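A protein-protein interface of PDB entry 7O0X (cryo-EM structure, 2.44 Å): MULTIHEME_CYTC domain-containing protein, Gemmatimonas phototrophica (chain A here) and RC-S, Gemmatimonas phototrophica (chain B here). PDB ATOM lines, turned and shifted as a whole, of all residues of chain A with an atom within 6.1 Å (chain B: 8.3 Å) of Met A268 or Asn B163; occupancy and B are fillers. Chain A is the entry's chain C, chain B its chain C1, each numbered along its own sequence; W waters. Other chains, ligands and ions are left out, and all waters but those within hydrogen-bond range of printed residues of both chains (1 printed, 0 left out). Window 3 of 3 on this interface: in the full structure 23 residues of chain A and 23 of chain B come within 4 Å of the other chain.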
ATOM      1  N   TYR A 162      -5.151  -6.773 -15.045  1.00  0.00           N
ATOM      2  CA  TYR A 162      -6.499  -6.390 -14.638  1.00  0.00           C
ATOM      3  C   TYR A 162      -6.566  -6.146 -13.135  1.00  0.00           C
ATOM      4  O   TYR A 162      -5.960  -6.872 -12.343  1.00  0.00           O
ATOM      5  CB  TYR A 162      -7.504  -7.482 -15.010  1.00  0.00           C
ATOM      6  CG  TYR A 162      -7.616  -7.777 -16.485  1.00  0.00           C
ATOM      7  CD1 TYR A 162      -7.562  -6.763 -17.427  1.00  0.00           C
ATOM      8  CD2 TYR A 162      -7.775  -9.079 -16.932  1.00  0.00           C
ATOM      9  CE1 TYR A 162      -7.697  -7.036 -18.772  1.00  0.00           C
ATOM     10  CE2 TYR A 162      -7.881  -9.364 -18.275  1.00  0.00           C
ATOM     11  CZ  TYR A 162      -7.848  -8.340 -19.191  1.00  0.00           C
ATOM     12  OH  TYR A 162      -7.921  -8.627 -20.531  1.00  0.00           O
ATOM     13  N   SER A 163      -7.320  -5.118 -12.745  1.00  0.00           N
ATOM     14  CA  SER A 163      -7.539  -4.829 -11.333  1.00  0.00           C
ATOM     15  C   SER A 163      -8.945  -4.292 -11.091  1.00  0.00           C
ATOM     16  O   SER A 163      -9.753  -4.937 -10.417  1.00  0.00           O
ATOM     17  CB  SER A 163      -6.491  -3.841 -10.816  1.00  0.00           C
ATOM     18  OG  SER A 163      -6.581  -2.598 -11.485  1.00  0.00           O
ATOM     19  N   SER A 164      -9.253  -3.123 -11.650  1.00  0.00           N
ATOM     20  CA  SER A 164     -10.575  -2.528 -11.544  1.00  0.00           C
ATOM     21  C   SER A 164     -11.041  -2.053 -12.915  1.00  0.00           C
ATOM     22  O   SER A 164     -10.238  -1.806 -13.816  1.00  0.00           O
ATOM     23  CB  SER A 164     -10.595  -1.367 -10.540  1.00  0.00           C
ATOM     24  OG  SER A 164      -9.873  -0.252 -11.024  1.00  0.00           O
ATOM     25  N   GLN A 165     -12.364  -1.940 -13.054  1.00  0.00           N
ATOM     26  CA  GLN A 165     -12.964  -1.503 -14.313  1.00  0.00           C
ATOM     27  C   GLN A 165     -12.463  -0.130 -14.751  1.00  0.00           C
ATOM     28  O   GLN A 165     -12.182   0.084 -15.936  1.00  0.00           O
ATOM     29  CB  GLN A 165     -14.486  -1.499 -14.179  1.00  0.00           C
ATOM     30  CG  GLN A 165     -15.078  -2.874 -13.909  1.00  0.00           C
ATOM     31  CD  GLN A 165     -16.589  -2.852 -13.779  1.00  0.00           C
ATOM     32  OE1 GLN A 165     -17.193  -1.800 -13.577  1.00  0.00           O
ATOM     33  NE2 GLN A 165     -17.207  -4.022 -13.888  1.00  0.00           N
ATOM     34  N   GLN A 257      -1.407 -15.665 -22.448  1.00  0.00           N
ATOM     35  CA  GLN A 257      -1.897 -16.196 -21.177  1.00  0.00           C
ATOM     36  C   GLN A 257      -1.702 -17.701 -20.974  1.00  0.00           C
ATOM     37  O   GLN A 257      -1.276 -18.088 -19.872  1.00  0.00           O
ATOM     38  CB  GLN A 257      -3.379 -15.815 -21.034  1.00  0.00           C
ATOM     39  CG  GLN A 257      -4.042 -16.307 -19.770  1.00  0.00           C
ATOM     40  CD  GLN A 257      -5.440 -15.750 -19.602  1.00  0.00           C
ATOM     41  OE1 GLN A 257      -5.713 -14.607 -19.968  1.00  0.00           O
ATOM     42  NE2 GLN A 257      -6.339 -16.558 -19.054  1.00  0.00           N
ATOM     43  N   GLY A 266      -1.325 -12.538 -13.643  1.00  0.00           N
ATOM     44  CA  GLY A 266      -1.985 -11.729 -12.641  1.00  0.00           C
ATOM     45  C   GLY A 266      -3.016 -12.503 -11.837  1.00  0.00           C
ATOM     46  O   GLY A 266      -3.308 -13.667 -12.102  1.00  0.00           O
ATOM     47  N   ALA A 267      -3.573 -11.826 -10.828  1.00  0.00           N
ATOM     48  CA  ALA A 267      -4.573 -12.459  -9.970  1.00  0.00           C
ATOM     49  C   ALA A 267      -5.834 -12.862 -10.727  1.00  0.00           C
ATOM     50  O   ALA A 267      -6.502 -13.826 -10.336  1.00  0.00           O
ATOM     51  CB  ALA A 267      -4.931 -11.522  -8.817  1.00  0.00           C
ATOM     52  N   MET A 268      -6.186 -12.150 -11.798  1.00  0.00           N
ATOM     53  CA  MET A 268      -7.251 -12.607 -12.686  1.00  0.00           C
ATOM     54  C   MET A 268      -6.798 -13.706 -13.638  1.00  0.00           C
ATOM     55  O   MET A 268      -7.584 -14.125 -14.494  1.00  0.00           O
ATOM     56  CB  MET A 268      -7.824 -11.435 -13.489  1.00  0.00           C
ATOM     57  CG  MET A 268      -8.309 -10.265 -12.648  1.00  0.00           C
ATOM     58  SD  MET A 268      -9.502 -10.742 -11.383  1.00  0.00           S
ATOM     59  CE  MET A 268     -10.951 -11.072 -12.386  1.00  0.00           C
ATOM     60  N   GLY A 269      -5.559 -14.178 -13.511  1.00  0.00           N
ATOM     61  CA  GLY A 269      -4.967 -15.090 -14.468  1.00  0.00           C
ATOM     62  C   GLY A 269      -4.619 -14.488 -15.809  1.00  0.00           C
ATOM     63  O   GLY A 269      -4.310 -15.234 -16.741  1.00  0.00           O
ATOM     64  N   ASP A 270      -4.659 -13.165 -15.938  1.00  0.00           N
ATOM     65  CA  ASP A 270      -4.352 -12.497 -17.193  1.00  0.00           C
ATOM     66  C   ASP A 270      -2.842 -12.342 -17.384  1.00  0.00           C
ATOM     67  O   ASP A 270      -2.064 -12.337 -16.428  1.00  0.00           O
ATOM     68  CB  ASP A 270      -5.050 -11.140 -17.262  1.00  0.00           C
ATOM     69  CG  ASP A 270      -4.596 -10.193 -16.177  1.00  0.00           C
ATOM     70  OD1 ASP A 270      -4.605 -10.588 -14.995  1.00  0.00           O
ATOM     71  OD2 ASP A 270      -4.246  -9.044 -16.509  1.00  0.00           O
ATOM     72  N   TYR B 156     -25.022  -3.228 -17.718  1.00  0.00           N
ATOM     73  CA  TYR B 156     -23.881  -3.276 -16.810  1.00  0.00           C
ATOM     74  C   TYR B 156     -23.836  -4.587 -16.032  1.00  0.00           C
ATOM     75  O   TYR B 156     -24.838  -4.997 -15.437  1.00  0.00           O
ATOM     76  CB  TYR B 156     -23.942  -2.101 -15.835  1.00  0.00           C
ATOM     77  CG  TYR B 156     -22.807  -2.067 -14.847  1.00  0.00           C
ATOM     78  CD1 TYR B 156     -21.514  -1.784 -15.260  1.00  0.00           C
ATOM     79  CD2 TYR B 156     -23.026  -2.324 -13.501  1.00  0.00           C
ATOM     80  CE1 TYR B 156     -20.473  -1.745 -14.360  1.00  0.00           C
ATOM     81  CE2 TYR B 156     -21.989  -2.293 -12.594  1.00  0.00           C
ATOM     82  CZ  TYR B 156     -20.715  -2.002 -13.029  1.00  0.00           C
ATOM     83  OH  TYR B 156     -19.674  -1.978 -12.133  1.00  0.00           O
ATOM     84  N   GLN B 158     -21.668  -6.257 -12.832  1.00  0.00           N
ATOM     85  CA  GLN B 158     -20.765  -5.939 -11.730  1.00  0.00           C
ATOM     86  C   GLN B 158     -19.484  -6.763 -11.790  1.00  0.00           C
ATOM     87  O   GLN B 158     -19.506  -7.951 -12.123  1.00  0.00           O
ATOM     88  CB  GLN B 158     -21.463  -6.197 -10.397  1.00  0.00           C
ATOM     89  CG  GLN B 158     -22.604  -5.257 -10.091  1.00  0.00           C
ATOM     90  CD  GLN B 158     -23.370  -5.672  -8.854  1.00  0.00           C
ATOM     91  OE1 GLN B 158     -24.515  -5.269  -8.655  1.00  0.00           O
ATOM     92  NE2 GLN B 158     -22.744  -6.490  -8.018  1.00  0.00           N
ATOM     93  N   ALA B 159     -18.365  -6.128 -11.447  1.00  0.00           N
ATOM     94  CA  ALA B 159     -17.140  -6.856 -11.157  1.00  0.00           C
ATOM     95  C   ALA B 159     -17.293  -7.666  -9.870  1.00  0.00           C
ATOM     96  O   ALA B 159     -18.134  -7.349  -9.026  1.00  0.00           O
ATOM     97  CB  ALA B 159     -15.967  -5.886 -11.035  1.00  0.00           C
ATOM     98  N   PRO B 160     -16.500  -8.729  -9.701  1.00  0.00           N
ATOM     99  CA  PRO B 160     -16.390  -9.364  -8.381  1.00  0.00           C
ATOM    100  C   PRO B 160     -16.044  -8.343  -7.305  1.00  0.00           C
ATOM    101  O   PRO B 160     -15.405  -7.324  -7.576  1.00  0.00           O
ATOM    102  CB  PRO B 160     -15.267 -10.390  -8.572  1.00  0.00           C
ATOM    103  CG  PRO B 160     -15.264 -10.673 -10.034  1.00  0.00           C
ATOM    104  CD  PRO B 160     -15.616  -9.369 -10.689  1.00  0.00           C
ATOM    105  N   ILE B 161     -16.470  -8.624  -6.070  1.00  0.00           N
ATOM    106  CA  ILE B 161     -16.328  -7.636  -5.003  1.00  0.00           C
ATOM    107  C   ILE B 161     -14.863  -7.291  -4.748  1.00  0.00           C
ATOM    108  O   ILE B 161     -14.540  -6.151  -4.393  1.00  0.00           O
ATOM    109  CB  ILE B 161     -17.041  -8.116  -3.719  1.00  0.00           C
ATOM    110  CG1 ILE B 161     -17.232  -6.944  -2.754  1.00  0.00           C
ATOM    111  CG2 ILE B 161     -16.288  -9.259  -3.054  1.00  0.00           C
ATOM    112  CD1 ILE B 161     -18.231  -7.206  -1.655  1.00  0.00           C
ATOM    113  N   THR B 162     -13.957  -8.253  -4.938  1.00  0.00           N
ATOM    114  CA  THR B 162     -12.522  -8.023  -4.805  1.00  0.00           C
ATOM    115  C   THR B 162     -11.923  -7.175  -5.922  1.00  0.00           C
ATOM    116  O   THR B 162     -10.752  -6.799  -5.819  1.00  0.00           O
ATOM    117  CB  THR B 162     -11.786  -9.361  -4.741  1.00  0.00           C
ATOM    118  OG1 THR B 162     -12.200 -10.188  -5.834  1.00  0.00           O
ATOM    119  CG2 THR B 162     -12.086 -10.069  -3.432  1.00  0.00           C
ATOM    120  N   ASN B 163     -12.676  -6.869  -6.973  1.00  0.00           N
ATOM    121  CA  ASN B 163     -12.236  -5.922  -7.989  1.00  0.00           C
ATOM    122  C   ASN B 163     -12.835  -4.533  -7.825  1.00  0.00           C
ATOM    123  O   ASN B 163     -12.522  -3.641  -8.618  1.00  0.00           O
ATOM    124  CB  ASN B 163     -12.569  -6.468  -9.380  1.00  0.00           C
ATOM    125  CG  ASN B 163     -11.812  -7.740  -9.699  1.00  0.00           C
ATOM    126  OD1 ASN B 163     -12.403  -8.809  -9.836  1.00  0.00           O
ATOM    127  ND2 ASN B 163     -10.494  -7.633  -9.811  1.00  0.00           N
ATOM    128  N   GLN B 164     -13.690  -4.328  -6.830  1.00  0.00           N
ATOM    129  CA  GLN B 164     -14.323  -3.039  -6.599  1.00  0.00           C
ATOM    130  C   GLN B 164     -13.453  -2.176  -5.690  1.00  0.00           C
ATOM    131  O   GLN B 164     -13.036  -2.621  -4.617  1.00  0.00           O
ATOM    132  CB  GLN B 164     -15.714  -3.244  -6.001  1.00  0.00           C
ATOM    133  CG  GLN B 164     -16.640  -4.018  -6.936  1.00  0.00           C
ATOM    134  CD  GLN B 164     -17.982  -4.342  -6.315  1.00  0.00           C
ATOM    135  OE1 GLN B 164     -18.469  -3.618  -5.454  1.00  0.00           O
ATOM    136  NE2 GLN B 164     -18.589  -5.441  -6.750  1.00  0.00           N
ATOM    137  N   ARG B 165     -13.169  -0.949  -6.129  1.00  0.00           N
ATOM    138  CA  ARG B 165     -12.416  -0.005  -5.312  1.00  0.00           C
ATOM    139  C   ARG B 165     -13.312   0.561  -4.221  1.00  0.00           C
ATOM    140  O   ARG B 165     -14.450   0.958  -4.483  1.00  0.00           O
ATOM    141  CB  ARG B 165     -11.914   1.157  -6.166  1.00  0.00           C
ATOM    142  CG  ARG B 165     -10.883   0.851  -7.225  1.00  0.00           C
ATOM    143  CD  ARG B 165     -10.502   2.160  -7.901  1.00  0.00           C
ATOM    144  NE  ARG B 165      -9.603   1.984  -9.033  1.00  0.00           N
ATOM    145  CZ  ARG B 165      -8.984   2.978  -9.656  1.00  0.00           C
ATOM    146  NH1 ARG B 165      -9.249   4.242  -9.372  1.00  0.00           N
ATOM    147  NH2 ARG B 165      -8.116   2.696 -10.622  1.00  0.00           N
ATOM    148  N   ARG B 166     -12.799   0.612  -2.997  1.00  0.00           N
ATOM    149  CA  ARG B 166     -13.530   1.294  -1.938  1.00  0.00           C
ATOM    150  C   ARG B 166     -13.220   2.788  -1.848  1.00  0.00           C
ATOM    151  O   ARG B 166     -13.962   3.516  -1.181  1.00  0.00           O
ATOM    152  CB  ARG B 166     -13.322   0.560  -0.601  1.00  0.00           C
ATOM    153  CG  ARG B 166     -12.188   0.977   0.280  1.00  0.00           C
ATOM    154  CD  ARG B 166     -11.704  -0.229   1.081  1.00  0.00           C
ATOM    155  NE  ARG B 166     -12.734  -0.845   1.910  1.00  0.00           N
ATOM    156  CZ  ARG B 166     -12.542  -1.921   2.663  1.00  0.00           C
ATOM    157  NH1 ARG B 166     -11.372  -2.536   2.707  1.00  0.00           N
ATOM    158  NH2 ARG B 166     -13.553  -2.397   3.383  1.00  0.00           N
ATOM    159  N   ARG B 189      -7.018  -1.168  -0.511  1.00  0.00           N
ATOM    160  CA  ARG B 189      -7.575  -0.507  -1.691  1.00  0.00           C
ATOM    161  C   ARG B 189      -8.843  -1.181  -2.206  1.00  0.00           C
ATOM    162  O   ARG B 189      -9.727  -0.500  -2.738  1.00  0.00           O
ATOM    163  CB  ARG B 189      -6.520  -0.451  -2.792  1.00  0.00           C
ATOM    164  CG  ARG B 189      -5.397   0.511  -2.480  1.00  0.00           C
ATOM    165  CD  ARG B 189      -4.292   0.451  -3.508  1.00  0.00           C
ATOM    166  NE  ARG B 189      -3.151   1.250  -3.084  1.00  0.00           N
ATOM    167  CZ  ARG B 189      -2.006   1.336  -3.743  1.00  0.00           C
ATOM    168  NH1 ARG B 189      -1.804   0.672  -4.867  1.00  0.00           N
ATOM    169  NH2 ARG B 189      -1.037   2.106  -3.259  1.00  0.00           N
ATOM    170  N   TYR B 190      -8.953  -2.497  -2.068  1.00  0.00           N
ATOM    171  CA  TYR B 190     -10.074  -3.262  -2.593  1.00  0.00           C
ATOM    172  C   TYR B 190     -10.861  -3.907  -1.460  1.00  0.00           C
ATOM    173  O   TYR B 190     -10.324  -4.164  -0.380  1.00  0.00           O
ATOM    174  CB  TYR B 190      -9.578  -4.301  -3.598  1.00  0.00           C
ATOM    175  CG  TYR B 190      -9.047  -3.631  -4.840  1.00  0.00           C
ATOM    176  CD1 TYR B 190      -9.907  -3.216  -5.843  1.00  0.00           C
ATOM    177  CD2 TYR B 190      -7.699  -3.333  -4.969  1.00  0.00           C
ATOM    178  CE1 TYR B 190      -9.431  -2.604  -6.982  1.00  0.00           C
ATOM    179  CE2 TYR B 190      -7.216  -2.692  -6.093  1.00  0.00           C
ATOM    180  CZ  TYR B 190      -8.087  -2.336  -7.098  1.00  0.00           C
ATOM    181  OH  TYR B 190      -7.616  -1.671  -8.204  1.00  0.00           O
ATOM    182  N   TYR B 191     -12.143  -4.156  -1.712  1.00  0.00           N
ATOM    183  CA  TYR B 191     -12.954  -4.894  -0.754  1.00  0.00           C
ATOM    184  C   TYR B 191     -12.471  -6.339  -0.640  1.00  0.00           C
ATOM    185  O   TYR B 191     -12.090  -6.949  -1.641  1.00  0.00           O
ATOM    186  CB  TYR B 191     -14.422  -4.874  -1.176  1.00  0.00           C
ATOM    187  CG  TYR B 191     -15.079  -3.526  -1.021  1.00  0.00           C
ATOM    188  CD1 TYR B 191     -15.601  -3.124   0.201  1.00  0.00           C
ATOM    189  CD2 TYR B 191     -15.171  -2.652  -2.094  1.00  0.00           C
ATOM    190  CE1 TYR B 191     -16.209  -1.895   0.345  1.00  0.00           C
ATOM    191  CE2 TYR B 191     -15.770  -1.418  -1.959  1.00  0.00           C
ATOM    192  CZ  TYR B 191     -16.290  -1.045  -0.737  1.00  0.00           C
ATOM    193  OH  TYR B 191     -16.876   0.190  -0.591  1.00  0.00           O
ATOM    194  N   PRO B 192     -12.473  -6.907   0.564  1.00  0.00           N
ATOM    195  CA  PRO B 192     -12.103  -8.315   0.717  1.00  0.00           C
ATOM    196  C   PRO B 192     -13.194  -9.247   0.210  1.00  0.00           C
ATOM    197  O   PRO B 192     -14.360  -8.873   0.069  1.00  0.00           O
ATOM    198  CB  PRO B 192     -11.896  -8.462   2.227  1.00  0.00           C
ATOM    199  CG  PRO B 192     -12.833  -7.470   2.811  1.00  0.00           C
ATOM    200  CD  PRO B 192     -12.842  -6.298   1.852  1.00  0.00           C
ATOM    201  N   ALA B 193     -12.781 -10.481  -0.077  1.00  0.00           N
ATOM    202  CA  ALA B 193     -13.711 -11.543  -0.442  1.00  0.00           C
ATOM    203  C   ALA B 193     -14.842 -11.675   0.571  1.00  0.00           C
ATOM    204  O   ALA B 193     -14.646 -11.489   1.775  1.00  0.00           O
ATOM    205  CB  ALA B 193     -12.962 -12.872  -0.567  1.00  0.00           C
HETATM  206  O   HOH W   1      -7.157  -0.100 -10.808  1.00  0.00           O
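Printed residues of chain B that touch a printed residue of chain A: Tyr B156, Ala B159, Asn B163, Arg B165 and Tyr B190.
Hydrophobic or aromatic side chains of chain B that line the printed part of chain A: Tyr B156, Ala B159 and Tyr B190.
Of the 10 printed residues of chain A, 4 touch a printed residue of chain B.
Printed residues of chain A that touch a printed residue of chain B: Ser A163, Ser A164, Gln A165 and Met A268.
Hydrophobic or aromatic side chains of chain A that line the printed part of chain B: Met A268.
Among the printed residues, 8 pairs touch across the chains.
Among the printed residues, no Asp or Glu carboxylate lies within 4 Å of a Lys or Arg side-chain nitrogen of the other chain.
Tyr B190 touches Ser A163.
Asn B163 touches Ser A164.
Tyr B190 touches Ser A164 (OH to CB, 3.8 Å).
Water W1 lies within hydrogen-bond range of the side-chain hydroxyl of Ser A163 (2.7 Å), the side-chain hydroxyl of Ser A164 (2.7 Å), the guanidinium group of Arg B165 (3.0 Å) and the side-chain hydroxyl of Tyr B190 (3.1 Å).
The side-chain amide nitrogen (ND2) of Asn B163 is in hydrogen-bond range of the backbone carbonyl oxygen (O) of Ser A163.
NE of Arg B165 lies within hydrogen-bond range of OG of Ser A164 (3.0 Å).
The side-chain hydroxyl (OH) of Tyr B156 sits at hydrogen-bond distance from the side-chain amide oxygen (OE1) of Gln A165.
NE2 of Gln A165 sits close to N of Ala B159 (3.4 Å).
The side-chain sulfur (SD) of Met A268 lies within hydrogen-bond range of the side-chain amide nitrogen (ND2) of Asn B163 (3.6 Å).
Printed residues of chain A within 4 Å of Asn B163: Ser A163 (2.9 Å), Ser A164 (3.5 Å) and Met A268 (3.6 Å).
No residue of chain B comes within 4 Å of Ala A267.
Printed residues of chain A within 4 Å of Arg B165: Ser A164 (3.0 Å).
Printed residues of chain B within 4 Å of Gln A165: Tyr B156 (2.9 Å) and Ala B159 (3.4 Å).
Of the printed residues of chain A, Tyr B156 touches Gln A165.
Of the printed residues of chain B, Ser A164 touches Asn B163, Arg B165 and Tyr B190.
Printed residues of chain A within 4 Å of Tyr B190: Ser A163 (3.6 Å) and Ser A164 (3.8 Å).
Asp A270 touches none of the printed residues of chain B.
The nearest residue of chain B that does not touch Met A268 is Pro B160 (4.9 Å).
The nearest residue of chain A that does not touch Asn B163 is Gln A165 (4.8 Å).
The backbone carbonyl oxygen (O) of Ala B159 lies within hydrogen-bond range of the side-chain amide nitrogen (NE2) of Gln B164 (3.0 Å).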
